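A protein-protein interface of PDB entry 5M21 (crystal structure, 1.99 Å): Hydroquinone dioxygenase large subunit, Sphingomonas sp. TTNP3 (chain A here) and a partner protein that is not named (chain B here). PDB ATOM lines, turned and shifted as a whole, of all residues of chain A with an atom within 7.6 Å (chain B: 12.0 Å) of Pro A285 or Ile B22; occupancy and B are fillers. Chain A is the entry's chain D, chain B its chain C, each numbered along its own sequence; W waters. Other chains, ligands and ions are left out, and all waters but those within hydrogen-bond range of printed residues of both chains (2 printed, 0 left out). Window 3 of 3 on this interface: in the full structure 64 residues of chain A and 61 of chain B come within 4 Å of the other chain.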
ATOM      1  N   ASP A 276     -17.305  16.671  13.372  1.00  0.00           N
ATOM      2  CA  ASP A 276     -16.357  16.976  12.293  1.00  0.00           C
ATOM      3  C   ASP A 276     -16.104  18.492  12.360  1.00  0.00           C
ATOM      4  O   ASP A 276     -17.026  19.262  12.205  1.00  0.00           O
ATOM      5  CB  ASP A 276     -16.928  16.529  10.933  1.00  0.00           C
ATOM      6  CG  ASP A 276     -15.936  16.762   9.762  1.00  0.00           C
ATOM      7  OD1 ASP A 276     -14.815  17.246   9.983  1.00  0.00           O
ATOM      8  OD2 ASP A 276     -16.270  16.493   8.594  1.00  0.00           O
ATOM      9  N   VAL A 277     -14.889  18.912  12.716  1.00  0.00           N
ATOM     10  CA  VAL A 277     -14.647  20.355  12.892  1.00  0.00           C
ATOM     11  C   VAL A 277     -13.859  20.960  11.731  1.00  0.00           C
ATOM     12  O   VAL A 277     -12.702  20.553  11.415  1.00  0.00           O
ATOM     13  CB  VAL A 277     -13.968  20.692  14.246  1.00  0.00           C
ATOM     14  CG1 VAL A 277     -13.806  22.209  14.390  1.00  0.00           C
ATOM     15  CG2 VAL A 277     -14.753  20.133  15.430  1.00  0.00           C
ATOM     16  N   LYS A 278     -14.496  21.929  11.080  1.00  0.00           N
ATOM     17  CA  LYS A 278     -13.886  22.583   9.947  1.00  0.00           C
ATOM     18  C   LYS A 278     -13.681  24.076  10.195  1.00  0.00           C
ATOM     19  O   LYS A 278     -14.375  24.669  11.003  1.00  0.00           O
ATOM     20  CB  LYS A 278     -14.694  22.328   8.663  1.00  0.00           C
ATOM     21  CG  LYS A 278     -14.893  20.841   8.343  1.00  0.00           C
ATOM     22  CD  LYS A 278     -15.347  20.642   6.935  1.00  0.00           C
ATOM     23  CE  LYS A 278     -15.489  19.154   6.645  1.00  0.00           C
ATOM     24  NZ  LYS A 278     -16.913  18.960   6.281  1.00  0.00           N
ATOM     25  N   ASP A 279     -12.737  24.677   9.489  1.00  0.00           N
ATOM     26  CA  ASP A 279     -12.636  26.132   9.514  1.00  0.00           C
ATOM     27  C   ASP A 279     -13.933  26.757   8.977  1.00  0.00           C
ATOM     28  O   ASP A 279     -14.488  26.326   7.963  1.00  0.00           O
ATOM     29  CB  ASP A 279     -11.436  26.571   8.711  1.00  0.00           C
ATOM     30  CG  ASP A 279     -11.170  28.033   8.873  1.00  0.00           C
ATOM     31  OD1 ASP A 279     -10.799  28.473   9.996  1.00  0.00           O
ATOM     32  OD2 ASP A 279     -11.376  28.752   7.881  1.00  0.00           O
ATOM     33  N   SER A 282     -13.064  28.712   5.399  1.00  0.00           N
ATOM     34  CA  SER A 282     -12.542  27.984   4.265  1.00  0.00           C
ATOM     35  C   SER A 282     -13.239  26.628   4.076  1.00  0.00           C
ATOM     36  O   SER A 282     -13.325  26.124   2.950  1.00  0.00           O
ATOM     37  CB  SER A 282     -11.047  27.785   4.420  1.00  0.00           C
ATOM     38  OG  SER A 282     -10.835  26.859   5.462  1.00  0.00           O
ATOM     39  N   GLY A 283     -13.730  26.035   5.165  1.00  0.00           N
ATOM     40  CA  GLY A 283     -14.255  24.638   5.098  1.00  0.00           C
ATOM     41  C   GLY A 283     -13.187  23.555   5.242  1.00  0.00           C
ATOM     42  O   GLY A 283     -13.475  22.380   5.090  1.00  0.00           O
ATOM     43  N   LYS A 284     -11.946  23.943   5.527  1.00  0.00           N
ATOM     44  CA  LYS A 284     -10.898  22.969   5.774  1.00  0.00           C
ATOM     45  C   LYS A 284     -11.043  22.234   7.091  1.00  0.00           C
ATOM     46  O   LYS A 284     -11.285  22.858   8.126  1.00  0.00           O
ATOM     47  CB  LYS A 284      -9.512  23.622   5.783  1.00  0.00           C
ATOM     48  CG  LYS A 284      -9.148  24.237   4.470  1.00  0.00           C
ATOM     49  CD  LYS A 284      -7.665  24.590   4.467  1.00  0.00           C
ATOM     50  CE  LYS A 284      -7.370  25.433   3.243  1.00  0.00           C
ATOM     51  NZ  LYS A 284      -5.895  25.428   3.062  1.00  0.00           N
ATOM     52  N   PRO A 285     -10.808  20.908   7.077  1.00  0.00           N
ATOM     53  CA  PRO A 285     -10.838  20.172   8.316  1.00  0.00           C
ATOM     54  C   PRO A 285      -9.764  20.675   9.295  1.00  0.00           C
ATOM     55  O   PRO A 285      -8.618  20.886   8.908  1.00  0.00           O
ATOM     56  CB  PRO A 285     -10.514  18.720   7.846  1.00  0.00           C
ATOM     57  CG  PRO A 285     -11.177  18.668   6.507  1.00  0.00           C
ATOM     58  CD  PRO A 285     -10.752  19.995   5.912  1.00  0.00           C
ATOM     59  N   ARG A 286     -10.154  20.865  10.554  1.00  0.00           N
ATOM     60  CA  ARG A 286      -9.210  21.244  11.580  1.00  0.00           C
ATOM     61  C   ARG A 286      -9.140  20.193  12.714  1.00  0.00           C
ATOM     62  O   ARG A 286      -8.095  19.988  13.332  1.00  0.00           O
ATOM     63  CB  ARG A 286      -9.576  22.633  12.113  1.00  0.00           C
ATOM     64  CG  ARG A 286      -9.173  23.744  11.138  1.00  0.00           C
ATOM     65  CD  ARG A 286      -9.744  25.108  11.495  1.00  0.00           C
ATOM     66  NE  ARG A 286      -9.601  25.436  12.905  1.00  0.00           N
ATOM     67  CZ  ARG A 286      -9.809  26.660  13.429  1.00  0.00           C
ATOM     68  NH1 ARG A 286     -10.161  27.678  12.674  1.00  0.00           N
ATOM     69  NH2 ARG A 286      -9.703  26.867  14.735  1.00  0.00           N
ATOM     70  N   ALA A 287     -10.248  19.540  13.026  1.00  0.00           N
ATOM     71  CA  ALA A 287     -10.235  18.714  14.202  1.00  0.00           C
ATOM     72  C   ALA A 287     -11.376  17.717  14.127  1.00  0.00           C
ATOM     73  O   ALA A 287     -12.275  17.911  13.346  1.00  0.00           O
ATOM     74  CB  ALA A 287     -10.366  19.603  15.463  1.00  0.00           C
ATOM     75  N   ARG A 288     -11.317  16.650  14.930  1.00  0.00           N
ATOM     76  CA  ARG A 288     -12.491  15.785  15.127  1.00  0.00           C
ATOM     77  C   ARG A 288     -12.657  15.569  16.636  1.00  0.00           C
ATOM     78  O   ARG A 288     -11.689  15.298  17.358  1.00  0.00           O
ATOM     79  CB  ARG A 288     -12.382  14.466  14.367  1.00  0.00           C
ATOM     80  CG  ARG A 288     -12.088  14.650  12.882  1.00  0.00           C
ATOM     81  CD  ARG A 288     -11.860  13.298  12.209  1.00  0.00           C
ATOM     82  NE  ARG A 288     -13.133  12.570  12.065  1.00  0.00           N
ATOM     83  CZ  ARG A 288     -13.497  11.498  12.772  1.00  0.00           C
ATOM     84  NH1 ARG A 288     -12.719  10.955  13.707  1.00  0.00           N
ATOM     85  NH2 ARG A 288     -14.655  10.935  12.507  1.00  0.00           N
ATOM     86  N   GLY B  18     -12.370  13.035  23.538  1.00  0.00           N
ATOM     87  CA  GLY B  18     -11.410  14.094  23.341  1.00  0.00           C
ATOM     88  C   GLY B  18     -11.297  14.593  21.899  1.00  0.00           C
ATOM     89  O   GLY B  18     -12.144  14.321  21.018  1.00  0.00           O
ATOM     90  N   VAL B  19     -10.236  15.370  21.706  1.00  0.00           N
ATOM     91  CA  VAL B  19      -9.996  16.120  20.527  1.00  0.00           C
ATOM     92  C   VAL B  19      -8.859  15.481  19.752  1.00  0.00           C
ATOM     93  O   VAL B  19      -7.774  15.295  20.308  1.00  0.00           O
ATOM     94  CB  VAL B  19      -9.629  17.575  20.908  1.00  0.00           C
ATOM     95  CG1 VAL B  19      -9.499  18.420  19.674  1.00  0.00           C
ATOM     96  CG2 VAL B  19     -10.709  18.159  21.828  1.00  0.00           C
ATOM     97  N   GLU B  20      -9.123  15.125  18.491  1.00  0.00           N
ATOM     98  CA  GLU B  20      -8.078  14.763  17.537  1.00  0.00           C
ATOM     99  C   GLU B  20      -7.875  15.946  16.621  1.00  0.00           C
ATOM    100  O   GLU B  20      -8.821  16.554  16.081  1.00  0.00           O
ATOM    101  CB  GLU B  20      -8.461  13.578  16.654  1.00  0.00           C
ATOM    102  CG  GLU B  20      -8.646  12.219  17.298  1.00  0.00           C
ATOM    103  CD  GLU B  20      -9.617  11.340  16.483  1.00  0.00           C
ATOM    104  OE1 GLU B  20     -10.352  10.573  17.134  1.00  0.00           O
ATOM    105  OE2 GLU B  20      -9.694  11.428  15.203  1.00  0.00           O
ATOM    106  N   ILE B  21      -6.614  16.229  16.380  1.00  0.00           N
ATOM    107  CA  ILE B  21      -6.224  17.445  15.748  1.00  0.00           C
ATOM    108  C   ILE B  21      -5.801  17.134  14.335  1.00  0.00           C
ATOM    109  O   ILE B  21      -4.959  16.255  14.102  1.00  0.00           O
ATOM    110  CB  ILE B  21      -5.028  18.078  16.546  1.00  0.00           C
ATOM    111  CG1 ILE B  21      -5.519  18.633  17.887  1.00  0.00           C
ATOM    112  CG2 ILE B  21      -4.318  19.141  15.723  1.00  0.00           C
ATOM    113  CD1 ILE B  21      -6.611  19.674  17.747  1.00  0.00           C
ATOM    114  N   ILE B  22      -6.373  17.869  13.392  1.00  0.00           N
ATOM    115  CA  ILE B  22      -5.814  17.898  12.058  1.00  0.00           C
ATOM    116  C   ILE B  22      -4.914  19.142  11.946  1.00  0.00           C
ATOM    117  O   ILE B  22      -3.717  19.035  11.678  1.00  0.00           O
ATOM    118  CB  ILE B  22      -6.903  17.759  10.959  1.00  0.00           C
ATOM    119  CG1 ILE B  22      -7.618  16.399  11.128  1.00  0.00           C
ATOM    120  CG2 ILE B  22      -6.278  17.855   9.563  1.00  0.00           C
ATOM    121  CD1 ILE B  22      -9.065  16.359  10.675  1.00  0.00           C
ATOM    122  N   ASP B  23      -5.481  20.314  12.194  1.00  0.00           N
ATOM    123  CA  ASP B  23      -4.710  21.550  12.197  1.00  0.00           C
ATOM    124  C   ASP B  23      -5.382  22.534  13.156  1.00  0.00           C
ATOM    125  O   ASP B  23      -6.255  23.289  12.753  1.00  0.00           O
ATOM    126  CB  ASP B  23      -4.651  22.113  10.760  1.00  0.00           C
ATOM    127  CG  ASP B  23      -3.710  23.316  10.616  1.00  0.00           C
ATOM    128  OD1 ASP B  23      -3.586  24.121  11.554  1.00  0.00           O
ATOM    129  OD2 ASP B  23      -3.108  23.489   9.540  1.00  0.00           O
ATOM    130  N   ASP B  24      -4.960  22.510  14.415  1.00  0.00           N
ATOM    131  CA  ASP B  24      -5.642  23.252  15.459  1.00  0.00           C
ATOM    132  C   ASP B  24      -4.944  23.033  16.777  1.00  0.00           C
ATOM    133  O   ASP B  24      -3.950  22.299  16.883  1.00  0.00           O
ATOM    134  CB  ASP B  24      -7.105  22.744  15.576  1.00  0.00           C
ATOM    135  CG  ASP B  24      -8.132  23.858  15.851  1.00  0.00           C
ATOM    136  OD1 ASP B  24      -7.778  24.870  16.520  1.00  0.00           O
ATOM    137  OD2 ASP B  24      -9.316  23.689  15.411  1.00  0.00           O
ATOM    138  N   ASP B  25      -5.516  23.628  17.807  1.00  0.00           N
ATOM    139  CA  ASP B  25      -5.040  23.509  19.179  1.00  0.00           C
ATOM    140  C   ASP B  25      -6.193  22.968  20.041  1.00  0.00           C
ATOM    141  O   ASP B  25      -7.307  23.489  20.019  1.00  0.00           O
ATOM    142  CB  ASP B  25      -4.604  24.901  19.652  1.00  0.00           C
ATOM    143  CG  ASP B  25      -4.079  24.929  21.081  1.00  0.00           C
ATOM    144  OD1 ASP B  25      -4.188  23.958  21.850  1.00  0.00           O
ATOM    145  OD2 ASP B  25      -3.548  25.993  21.423  1.00  0.00           O
ATOM    146  N   PRO B  26      -5.933  21.877  20.748  1.00  0.00           N
ATOM    147  CA  PRO B  26      -6.993  21.239  21.518  1.00  0.00           C
ATOM    148  C   PRO B  26      -7.547  22.145  22.605  1.00  0.00           C
ATOM    149  O   PRO B  26      -8.735  22.053  22.913  1.00  0.00           O
ATOM    150  CB  PRO B  26      -6.315  19.984  22.106  1.00  0.00           C
ATOM    151  CG  PRO B  26      -4.822  20.193  21.905  1.00  0.00           C
ATOM    152  CD  PRO B  26      -4.721  21.047  20.667  1.00  0.00           C
ATOM    153  N   ARG B  27      -6.708  23.023  23.175  1.00  0.00           N
ATOM    154  CA  ARG B  27      -7.194  24.029  24.166  1.00  0.00           C
ATOM    155  C   ARG B  27      -8.301  24.952  23.635  1.00  0.00           C
ATOM    156  O   ARG B  27      -9.067  25.511  24.443  1.00  0.00           O
ATOM    157  CB  ARG B  27      -6.052  24.858  24.766  1.00  0.00           C
ATOM    158  CG  ARG B  27      -4.752  24.091  24.870  1.00  0.00           C
ATOM    159  CD  ARG B  27      -3.569  25.032  25.003  1.00  0.00           C
ATOM    160  NE  ARG B  27      -3.229  25.119  26.411  1.00  0.00           N
ATOM    161  CZ  ARG B  27      -2.142  24.573  26.937  1.00  0.00           C
ATOM    162  NH1 ARG B  27      -1.271  23.934  26.142  1.00  0.00           N
ATOM    163  NH2 ARG B  27      -1.920  24.686  28.250  1.00  0.00           N
ATOM    164  N   ASN B  28      -8.419  25.098  22.308  1.00  0.00           N
ATOM    165  CA  ASN B  28      -9.562  25.836  21.747  1.00  0.00           C
ATOM    166  C   ASN B  28     -10.936  25.209  22.061  1.00  0.00           C
ATOM    167  O   ASN B  28     -11.969  25.895  21.944  1.00  0.00           O
ATOM    168  CB  ASN B  28      -9.445  26.025  20.227  1.00  0.00           C
ATOM    169  CG  ASN B  28      -8.235  26.838  19.843  1.00  0.00           C
ATOM    170  OD1 ASN B  28      -7.664  27.537  20.661  1.00  0.00           O
ATOM    171  ND2 ASN B  28      -7.819  26.710  18.619  1.00  0.00           N
ATOM    172  N   TYR B  29     -10.947  23.928  22.443  1.00  0.00           N
ATOM    173  CA  TYR B  29     -12.221  23.154  22.606  1.00  0.00           C
ATOM    174  C   TYR B  29     -12.597  22.902  24.078  1.00  0.00           C
ATOM    175  O   TYR B  29     -13.660  22.302  24.360  1.00  0.00           O
ATOM    176  CB  TYR B  29     -12.183  21.831  21.801  1.00  0.00           C
ATOM    177  CG  TYR B  29     -11.980  22.132  20.343  1.00  0.00           C
ATOM    178  CD1 TYR B  29     -13.071  22.416  19.536  1.00  0.00           C
ATOM    179  CD2 TYR B  29     -10.704  22.238  19.789  1.00  0.00           C
ATOM    180  CE1 TYR B  29     -12.913  22.726  18.204  1.00  0.00           C
ATOM    181  CE2 TYR B  29     -10.529  22.587  18.442  1.00  0.00           C
ATOM    182  CZ  TYR B  29     -11.654  22.827  17.659  1.00  0.00           C
ATOM    183  OH  TYR B  29     -11.596  23.190  16.317  1.00  0.00           O
ATOM    184  N   GLN B 166      -8.359  19.164  28.200  1.00  0.00           N
ATOM    185  CA  GLN B 166      -7.288  18.545  27.402  1.00  0.00           C
ATOM    186  C   GLN B 166      -6.355  19.638  26.904  1.00  0.00           C
ATOM    187  O   GLN B 166      -6.809  20.658  26.372  1.00  0.00           O
ATOM    188  CB  GLN B 166      -7.907  17.789  26.235  1.00  0.00           C
ATOM    189  CG  GLN B 166      -6.934  17.037  25.355  1.00  0.00           C
ATOM    190  CD  GLN B 166      -7.648  16.361  24.221  1.00  0.00           C
ATOM    191  OE1 GLN B 166      -8.825  16.001  24.331  1.00  0.00           O
ATOM    192  NE2 GLN B 166      -6.959  16.225  23.100  1.00  0.00           N
ATOM    193  N   GLU B 168      -2.983  18.619  25.490  1.00  0.00           N
ATOM    194  CA  GLU B 168      -2.192  18.018  24.407  1.00  0.00           C
ATOM    195  C   GLU B 168      -3.055  17.155  23.480  1.00  0.00           C
ATOM    196  O   GLU B 168      -4.189  16.801  23.827  1.00  0.00           O
ATOM    197  CB  GLU B 168      -1.054  17.150  24.986  1.00  0.00           C
ATOM    198  CG  GLU B 168      -0.209  17.847  26.040  1.00  0.00           C
ATOM    199  CD  GLU B 168       0.619  18.999  25.482  1.00  0.00           C
ATOM    200  OE1 GLU B 168       0.863  19.051  24.244  1.00  0.00           O
ATOM    201  OE2 GLU B 168       1.036  19.861  26.290  1.00  0.00           O
ATOM    202  N   ALA B 169      -2.503  16.799  22.325  1.00  0.00           N
ATOM    203  CA  ALA B 169      -3.118  15.763  21.475  1.00  0.00           C
ATOM    204  C   ALA B 169      -2.066  14.885  20.828  1.00  0.00           C
ATOM    205  O   ALA B 169      -1.006  15.397  20.478  1.00  0.00           O
ATOM    206  CB  ALA B 169      -4.006  16.381  20.419  1.00  0.00           C
HETATM  207  O   HOH W   1     -10.413  28.376  17.390  1.00  0.00           O
HETATM  208  O   HOH W   2     -12.103  12.275  17.981  1.00  0.00           O
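The side-chain carboxylate (OE2) of Glu B20 is in salt-bridge range of the guanidinium group (NH1) of Arg A288 (3.4 Å).
O of Arg A286 is in hydrogen-bond range of N of Ile B22, at 2.7 Å.
N of Asp B23 is in hydrogen-bond range of O of Arg A286, at 2.9 Å.
The side-chain carboxylate (OD2) of Asp B24 is in salt-bridge range of the guanidinium group (NE) of Arg A286.
Of the 11 printed residues of chain A, 5 touch a printed residue of chain B.
Hydrophobic or aromatic side chains of chain B within 4 Å of the printed part of chain A: Ile B22 and Tyr B29.
Among the printed residues, Asp or Glu carboxylates within 4 Å of a Lys or Arg side-chain nitrogen of the other chain: Arg A286 with Asp B24 and Arg A288 with Glu B20.
The backbone NH (N) of Val B19 is in hydrogen-bond range of the side-chain amide oxygen (OE1) of Gln B166.
OD1 of Asp B24 lies within hydrogen-bond range of ND2 of Asn B28 (2.8 Å).
The side-chain hydroxyl of Tyr B29 lies within hydrogen-bond range of the side-chain carboxylate of Asp B24.
The backbone carbonyl oxygen (O) of Val A277 is in hydrogen-bond range of the backbone NH (N) of Arg A286 (2.7 Å).
N of Val A277 is in hydrogen-bond range of O of Ala A287.
OD1 of Asp A279 is in salt-bridge range of NH1 of Arg A286 (2.9 Å).
Water W2 lies within hydrogen-bond range of OE1 of Glu B20 (2.6 Å) and O of Arg A288 (3.1 Å).
Water W1 bridges NH2 of Arg A286 and ND2 of Asn B28.
OH of Tyr B29 touches CG1 of Val A277, 3.1 Å away.
Pro A285 touches Ile B22 (O to CG2, 3.9 Å).
Ile B21 touches Arg A286.
Glu B20 touches Ala A287 (O to CA, 3.2 Å).
CB of Ala A287 touches OH of Tyr B29 (3.9 Å).
Arg A288 touches Gly B18.
Val B19 touches Arg A288 (CA to O, 3.7 Å).
Of chain B, only Ile B22 comes within 4 Å of Pro A285.
Of chain A, only Pro A285 and Arg A286 come within 4 Å of Ile B22.
Of chain B, only Tyr B29 (3.1 Å) comes within 4 Å of Val A277.
No residue of chain B comes within 4 Å of Lys A278.
No residue of chain B comes within 4 Å of Asp A279.
No residue of chain B comes within 4 Å of Gly A283.
Ala A287 touches two residues of chain B.
Of the printed residues of chain A, Val B19 touches Arg A288 (3.7 Å).
Printed residues of chain A within 4 Å of Asp B23: Arg A286 (2.9 Å).
Of the printed residues of chain A, Tyr B29 touches Val A277 (3.1 Å) and Ala A287 (3.9 Å).
Printed residues of chain B within 4 Å of Arg A288: Gly B18 (3.8 Å), Val B19 (3.7 Å) and Glu B20 (2.8 Å).
Of the printed residues of chain A, Asp B24 touches Arg A286.
The nearest residue of chain B that does not touch Pro A285 is Asp B23 (4.5 Å).
The nearest residue of chain A that does not touch Ile B22 is Ala A287 (4.04 Å).
The nearest printed residue of chain A that does not touch Ile B21 is Ala A287 (4.4 Å).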
